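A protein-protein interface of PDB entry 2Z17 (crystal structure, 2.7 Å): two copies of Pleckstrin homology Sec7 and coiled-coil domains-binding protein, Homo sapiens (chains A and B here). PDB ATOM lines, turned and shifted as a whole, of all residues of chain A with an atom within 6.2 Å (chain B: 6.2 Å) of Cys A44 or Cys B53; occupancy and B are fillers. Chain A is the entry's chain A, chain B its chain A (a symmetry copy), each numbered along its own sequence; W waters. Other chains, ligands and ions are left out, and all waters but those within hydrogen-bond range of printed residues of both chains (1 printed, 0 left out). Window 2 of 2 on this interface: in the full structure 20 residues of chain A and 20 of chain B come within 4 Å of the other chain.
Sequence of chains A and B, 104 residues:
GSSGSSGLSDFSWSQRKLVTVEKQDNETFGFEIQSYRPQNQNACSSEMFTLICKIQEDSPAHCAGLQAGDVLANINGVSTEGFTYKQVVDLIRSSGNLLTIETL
The backbone NH (N) of Phe A11 lies close to the side-chain amino group (NZ) of Lys B54, 3.0 Å away.
The side-chain sulfur (SG) of Cys A44 lies close to the side-chain sulfur (SG) of Cys B53.
N of Glu B32 is in hydrogen-bond range of O of Lys B54, at 2.8 Å.
O of Ile B33 sits at hydrogen-bond distance from SG of Cys B53 (3.3 Å).
The backbone carbonyl oxygen (O) of Leu B51 lies within hydrogen-bond range of the backbone NH (N) of Gln B34, at 2.9 Å.
The backbone carbonyl oxygen (O) of Glu B32 sits at hydrogen-bond distance from the backbone NH (N) of Cys B53 (2.5 Å).
The side-chain amide oxygen of Asn A42 sits at hydrogen-bond distance from the backbone NH of Cys A44 (2.9 Å).
Among the printed residues, merely in contact across the chains: Asn A42 with Ile B33, Phe A11 with Cys B53, Ala A43 with Glu B32, Phe A11 with Ala B68 and Asn A42 with Gln B34.
Cys A44 touches one residue of chain B.
Cys B53 touches just these residues of chain A: Phe A11 and Cys A44.
Of the printed residues of chain A, Ala B68 touches Phe A11 (3.8 Å).
Printed residues of chain B within 4 Å of Asn A42: Ile B33 and Gln B34.
Printed residues of chain B within 4 Å of Phe A11: Cys B53 (3.7 Å), Lys B54 (3.0 Å) and Ala B68 (3.8 Å).
The nearest residue of chain A that does not touch Cys B53 is Asn A42 (4.7 Å).
The nearest printed residue of chain B that does not touch Ala A43 is Lys B54 (5.4 Å).
Of the 8 printed residues of chain A, 4 touch a printed residue of chain B.
Printed residues of chain A that touch a printed residue of chain B: Phe A11, Asn A42, Ala A43 and Cys A44.
Hydrophobic or aromatic side chains of chain B that line the printed part of chain A: Ala B68.
Among the printed residues, 7 pairs touch across the chains.
Among the printed residues, no Asp or Glu carboxylate lies within 4 Å of a Lys or Arg side-chain nitrogen of the other chain.
No position is printed for both chains.
Water W1 lies within hydrogen-bond range of NZ of Lys B54 (3.4 Å) and OG of Ser A45 (3.5 Å).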
ATOM      1  N   PHE A  11     -15.671 -22.753  26.253  1.00  0.00           N
ATOM      2  CA  PHE A  11     -17.076 -22.784  26.752  1.00  0.00           C
ATOM      3  C   PHE A  11     -18.063 -22.421  25.644  1.00  0.00           C
ATOM      4  O   PHE A  11     -18.970 -23.209  25.319  1.00  0.00           O
ATOM      5  CB  PHE A  11     -17.246 -21.808  27.922  1.00  0.00           C
ATOM      6  CG  PHE A  11     -18.510 -22.024  28.695  1.00  0.00           C
ATOM      7  CD1 PHE A  11     -19.752 -21.759  28.113  1.00  0.00           C
ATOM      8  CD2 PHE A  11     -18.467 -22.563  29.978  1.00  0.00           C
ATOM      9  CE1 PHE A  11     -20.924 -22.029  28.788  1.00  0.00           C
ATOM     10  CE2 PHE A  11     -19.633 -22.841  30.666  1.00  0.00           C
ATOM     11  CZ  PHE A  11     -20.870 -22.573  30.067  1.00  0.00           C
ATOM     12  N   SER A  12     -17.878 -21.215  25.096  1.00  0.00           N
ATOM     13  CA  SER A  12     -18.698 -20.669  24.008  1.00  0.00           C
ATOM     14  C   SER A  12     -20.010 -21.434  23.786  1.00  0.00           C
ATOM     15  O   SER A  12     -20.134 -22.268  22.887  1.00  0.00           O
ATOM     16  CB  SER A  12     -17.865 -20.610  22.708  1.00  0.00           C
ATOM     17  OG  SER A  12     -16.906 -21.657  22.650  1.00  0.00           O
ATOM     18  N   GLN A  41      -7.576 -32.276  35.009  1.00  0.00           N
ATOM     19  CA  GLN A  41      -6.702 -31.165  34.738  1.00  0.00           C
ATOM     20  C   GLN A  41      -6.310 -31.343  33.280  1.00  0.00           C
ATOM     21  O   GLN A  41      -5.980 -32.458  32.860  1.00  0.00           O
ATOM     22  CB  GLN A  41      -5.484 -31.271  35.639  1.00  0.00           C
ATOM     23  CG  GLN A  41      -4.955 -32.711  35.728  1.00  0.00           C
ATOM     24  CD  GLN A  41      -5.665 -33.590  36.761  1.00  0.00           C
ATOM     25  OE1 GLN A  41      -6.881 -33.754  36.742  1.00  0.00           O
ATOM     26  NE2 GLN A  41      -4.884 -34.168  37.667  1.00  0.00           N
ATOM     27  N   ASN A  42      -6.390 -30.257  32.514  1.00  0.00           N
ATOM     28  CA  ASN A  42      -6.057 -30.249  31.093  1.00  0.00           C
ATOM     29  C   ASN A  42      -6.222 -28.838  30.529  1.00  0.00           C
ATOM     30  O   ASN A  42      -6.371 -27.877  31.285  1.00  0.00           O
ATOM     31  CB  ASN A  42      -6.937 -31.229  30.302  1.00  0.00           C
ATOM     32  CG  ASN A  42      -8.412 -30.925  30.432  1.00  0.00           C
ATOM     33  OD1 ASN A  42      -8.828 -29.770  30.328  1.00  0.00           O
ATOM     34  ND2 ASN A  42      -9.219 -31.963  30.649  1.00  0.00           N
ATOM     35  N   ALA A  43      -6.199 -28.740  29.199  1.00  0.00           N
ATOM     36  CA  ALA A  43      -6.302 -27.483  28.444  1.00  0.00           C
ATOM     37  C   ALA A  43      -7.440 -26.524  28.787  1.00  0.00           C
ATOM     38  O   ALA A  43      -7.444 -25.380  28.349  1.00  0.00           O
ATOM     39  CB  ALA A  43      -6.341 -27.803  26.957  1.00  0.00           C
ATOM     40  N   CYS A  44      -8.400 -26.975  29.576  1.00  0.00           N
ATOM     41  CA  CYS A  44      -9.525 -26.128  29.925  1.00  0.00           C
ATOM     42  C   CYS A  44      -9.398 -25.483  31.284  1.00  0.00           C
ATOM     43  O   CYS A  44      -8.428 -24.775  31.575  1.00  0.00           O
ATOM     44  CB  CYS A  44     -10.794 -26.948  29.855  1.00  0.00           C
ATOM     45  SG  CYS A  44     -10.931 -27.716  28.255  1.00  0.00           S
ATOM     46  N   SER A  45     -10.391 -25.711  32.125  1.00  0.00           N
ATOM     47  CA  SER A  45     -10.341 -25.122  33.440  1.00  0.00           C
ATOM     48  C   SER A  45     -11.173 -25.846  34.466  1.00  0.00           C
ATOM     49  O   SER A  45     -12.305 -26.240  34.223  1.00  0.00           O
ATOM     50  CB  SER A  45     -10.719 -23.641  33.367  1.00  0.00           C
ATOM     51  OG  SER A  45      -9.763 -22.922  32.588  1.00  0.00           O
ATOM     52  N   SER A  46     -10.541 -26.005  35.619  1.00  0.00           N
ATOM     53  CA  SER A  46     -11.052 -26.681  36.797  1.00  0.00           C
ATOM     54  C   SER A  46     -12.000 -25.866  37.684  1.00  0.00           C
ATOM     55  O   SER A  46     -12.274 -24.691  37.429  1.00  0.00           O
ATOM     56  CB  SER A  46      -9.841 -27.110  37.607  1.00  0.00           C
ATOM     57  OG  SER A  46      -8.814 -26.135  37.450  1.00  0.00           O
ATOM     58  N   PHE B  31     -10.940 -31.833  19.672  1.00  0.00           N
ATOM     59  CA  PHE B  31     -11.802 -31.440  20.775  1.00  0.00           C
ATOM     60  C   PHE B  31     -11.207 -31.860  22.089  1.00  0.00           C
ATOM     61  O   PHE B  31     -10.272 -32.656  22.125  1.00  0.00           O
ATOM     62  CB  PHE B  31     -13.187 -32.071  20.624  1.00  0.00           C
ATOM     63  CG  PHE B  31     -13.187 -33.582  20.568  1.00  0.00           C
ATOM     64  CD1 PHE B  31     -13.128 -34.339  21.722  1.00  0.00           C
ATOM     65  CD2 PHE B  31     -13.315 -34.246  19.352  1.00  0.00           C
ATOM     66  CE1 PHE B  31     -13.209 -35.741  21.671  1.00  0.00           C
ATOM     67  CE2 PHE B  31     -13.390 -35.652  19.301  1.00  0.00           C
ATOM     68  CZ  PHE B  31     -13.339 -36.389  20.465  1.00  0.00           C
ATOM     69  N   GLU B  32     -11.770 -31.328  23.166  1.00  0.00           N
ATOM     70  CA  GLU B  32     -11.321 -31.622  24.520  1.00  0.00           C
ATOM     71  C   GLU B  32     -12.504 -32.098  25.377  1.00  0.00           C
ATOM     72  O   GLU B  32     -13.608 -31.529  25.313  1.00  0.00           O
ATOM     73  CB  GLU B  32     -10.755 -30.356  25.129  1.00  0.00           C
ATOM     74  CG  GLU B  32      -9.649 -29.742  24.321  1.00  0.00           C
ATOM     75  CD  GLU B  32      -8.315 -30.380  24.619  1.00  0.00           C
ATOM     76  OE1 GLU B  32      -7.313 -29.931  24.023  1.00  0.00           O
ATOM     77  OE2 GLU B  32      -8.275 -31.325  25.450  1.00  0.00           O
ATOM     78  N   ILE B  33     -12.298 -33.142  26.172  1.00  0.00           N
ATOM     79  CA  ILE B  33     -13.393 -33.557  27.007  1.00  0.00           C
ATOM     80  C   ILE B  33     -13.199 -33.233  28.467  1.00  0.00           C
ATOM     81  O   ILE B  33     -12.161 -32.712  28.884  1.00  0.00           O
ATOM     82  CB  ILE B  33     -13.758 -35.039  26.857  1.00  0.00           C
ATOM     83  CG1 ILE B  33     -12.592 -35.914  27.266  1.00  0.00           C
ATOM     84  CG2 ILE B  33     -14.257 -35.301  25.451  1.00  0.00           C
ATOM     85  CD1 ILE B  33     -12.968 -37.377  27.275  1.00  0.00           C
ATOM     86  N   GLN B  34     -14.201 -33.578  29.263  1.00  0.00           N
ATOM     87  CA  GLN B  34     -14.162 -33.212  30.646  1.00  0.00           C
ATOM     88  C   GLN B  34     -15.180 -33.984  31.434  1.00  0.00           C
ATOM     89  O   GLN B  34     -16.354 -33.869  31.179  1.00  0.00           O
ATOM     90  CB  GLN B  34     -14.478 -31.719  30.693  1.00  0.00           C
ATOM     91  CG  GLN B  34     -13.405 -30.890  31.247  1.00  0.00           C
ATOM     92  CD  GLN B  34     -13.133 -31.298  32.641  1.00  0.00           C
ATOM     93  OE1 GLN B  34     -12.040 -31.088  33.171  1.00  0.00           O
ATOM     94  NE2 GLN B  34     -14.139 -31.903  33.268  1.00  0.00           N
ATOM     95  N   TYR B  36     -17.520 -34.646  34.591  1.00  0.00           N
ATOM     96  CA  TYR B  36     -18.056 -33.825  35.672  1.00  0.00           C
ATOM     97  C   TYR B  36     -18.864 -34.622  36.624  1.00  0.00           C
ATOM     98  O   TYR B  36     -19.784 -35.295  36.207  1.00  0.00           O
ATOM     99  CB  TYR B  36     -18.950 -32.711  35.161  1.00  0.00           C
ATOM    100  CG  TYR B  36     -18.199 -31.700  34.377  1.00  0.00           C
ATOM    101  CD1 TYR B  36     -17.949 -31.900  33.017  1.00  0.00           C
ATOM    102  CD2 TYR B  36     -17.668 -30.573  34.998  1.00  0.00           C
ATOM    103  CE1 TYR B  36     -17.193 -31.025  32.301  1.00  0.00           C
ATOM    104  CE2 TYR B  36     -16.897 -29.674  34.283  1.00  0.00           C
ATOM    105  CZ  TYR B  36     -16.656 -29.907  32.928  1.00  0.00           C
ATOM    106  OH  TYR B  36     -15.857 -29.037  32.198  1.00  0.00           O
ATOM    107  N   LEU B  51     -18.195 -34.103  28.867  1.00  0.00           N
ATOM    108  CA  LEU B  51     -18.587 -33.105  27.885  1.00  0.00           C
ATOM    109  C   LEU B  51     -17.409 -32.576  27.063  1.00  0.00           C
ATOM    110  O   LEU B  51     -16.277 -32.560  27.520  1.00  0.00           O
ATOM    111  CB  LEU B  51     -19.282 -31.940  28.603  1.00  0.00           C
ATOM    112  CG  LEU B  51     -18.889 -30.469  28.373  1.00  0.00           C
ATOM    113  CD1 LEU B  51     -19.935 -29.642  29.091  1.00  0.00           C
ATOM    114  CD2 LEU B  51     -17.486 -30.116  28.884  1.00  0.00           C
ATOM    115  N   ILE B  52     -17.682 -32.155  25.837  1.00  0.00           N
ATOM    116  CA  ILE B  52     -16.645 -31.577  25.003  1.00  0.00           C
ATOM    117  C   ILE B  52     -16.468 -30.201  25.636  1.00  0.00           C
ATOM    118  O   ILE B  52     -17.459 -29.535  25.929  1.00  0.00           O
ATOM    119  CB  ILE B  52     -17.141 -31.423  23.554  1.00  0.00           C
ATOM    120  CG1 ILE B  52     -17.419 -32.807  22.958  1.00  0.00           C
ATOM    121  CG2 ILE B  52     -16.126 -30.661  22.734  1.00  0.00           C
ATOM    122  CD1 ILE B  52     -17.809 -32.792  21.483  1.00  0.00           C
ATOM    123  N   CYS B  53     -15.240 -29.770  25.895  1.00  0.00           N
ATOM    124  CA  CYS B  53     -15.088 -28.443  26.498  1.00  0.00           C
ATOM    125  C   CYS B  53     -14.433 -27.443  25.563  1.00  0.00           C
ATOM    126  O   CYS B  53     -14.642 -26.242  25.688  1.00  0.00           O
ATOM    127  CB  CYS B  53     -14.340 -28.497  27.857  1.00  0.00           C
ATOM    128  SG  CYS B  53     -12.871 -29.571  28.032  1.00  0.00           S
ATOM    129  N   LYS B  54     -13.660 -27.942  24.606  1.00  0.00           N
ATOM    130  CA  LYS B  54     -12.997 -27.062  23.657  1.00  0.00           C
ATOM    131  C   LYS B  54     -12.955 -27.701  22.274  1.00  0.00           C
ATOM    132  O   LYS B  54     -12.744 -28.911  22.139  1.00  0.00           O
ATOM    133  CB  LYS B  54     -11.569 -26.749  24.121  1.00  0.00           C
ATOM    134  CG  LYS B  54     -11.288 -25.276  24.317  1.00  0.00           C
ATOM    135  CD  LYS B  54     -12.303 -24.650  25.265  1.00  0.00           C
ATOM    136  CE  LYS B  54     -11.818 -23.304  25.849  1.00  0.00           C
ATOM    137  NZ  LYS B  54     -12.709 -22.818  26.965  1.00  0.00           N
ATOM    138  N   ILE B  55     -13.159 -26.872  21.255  1.00  0.00           N
ATOM    139  CA  ILE B  55     -13.123 -27.325  19.892  1.00  0.00           C
ATOM    140  C   ILE B  55     -12.186 -26.460  19.083  1.00  0.00           C
ATOM    141  O   ILE B  55     -12.301 -25.260  19.085  1.00  0.00           O
ATOM    142  CB  ILE B  55     -14.512 -27.306  19.288  1.00  0.00           C
ATOM    143  CG1 ILE B  55     -15.372 -28.322  20.041  1.00  0.00           C
ATOM    144  CG2 ILE B  55     -14.455 -27.650  17.800  1.00  0.00           C
ATOM    145  CD1 ILE B  55     -16.681 -28.699  19.354  1.00  0.00           C
ATOM    146  N   ALA B  68     -18.830 -27.399  21.575  1.00  0.00           N
ATOM    147  CA  ALA B  68     -18.488 -27.415  22.999  1.00  0.00           C
ATOM    148  C   ALA B  68     -19.770 -27.323  23.808  1.00  0.00           C
ATOM    149  O   ALA B  68     -20.498 -26.350  23.702  1.00  0.00           O
ATOM    150  CB  ALA B  68     -17.577 -26.262  23.334  1.00  0.00           C
ATOM    151  N   GLY B  69     -20.026 -28.342  24.616  1.00  0.00           N
ATOM    152  CA  GLY B  69     -21.233 -28.406  25.395  1.00  0.00           C
ATOM    153  C   GLY B  69     -21.872 -29.743  25.082  1.00  0.00           C
ATOM    154  O   GLY B  69     -22.698 -30.254  25.856  1.00  0.00           O
ATOM    155  N   ASP B  70     -21.488 -30.319  23.936  1.00  0.00           N
ATOM    156  CA  ASP B  70     -22.012 -31.613  23.499  1.00  0.00           C
ATOM    157  C   ASP B  70     -21.714 -32.675  24.555  1.00  0.00           C
ATOM    158  O   ASP B  70     -20.596 -32.719  25.076  1.00  0.00           O
ATOM    159  CB  ASP B  70     -21.362 -32.044  22.182  1.00  0.00           C
ATOM    160  CG  ASP B  70     -22.116 -31.552  20.953  1.00  0.00           C
ATOM    161  OD1 ASP B  70     -23.368 -31.588  20.994  1.00  0.00           O
ATOM    162  OD2 ASP B  70     -21.466 -31.155  19.944  1.00  0.00           O
HETATM  163  O   HOH W   1     -12.426 -23.193  30.362  1.00  0.00           O
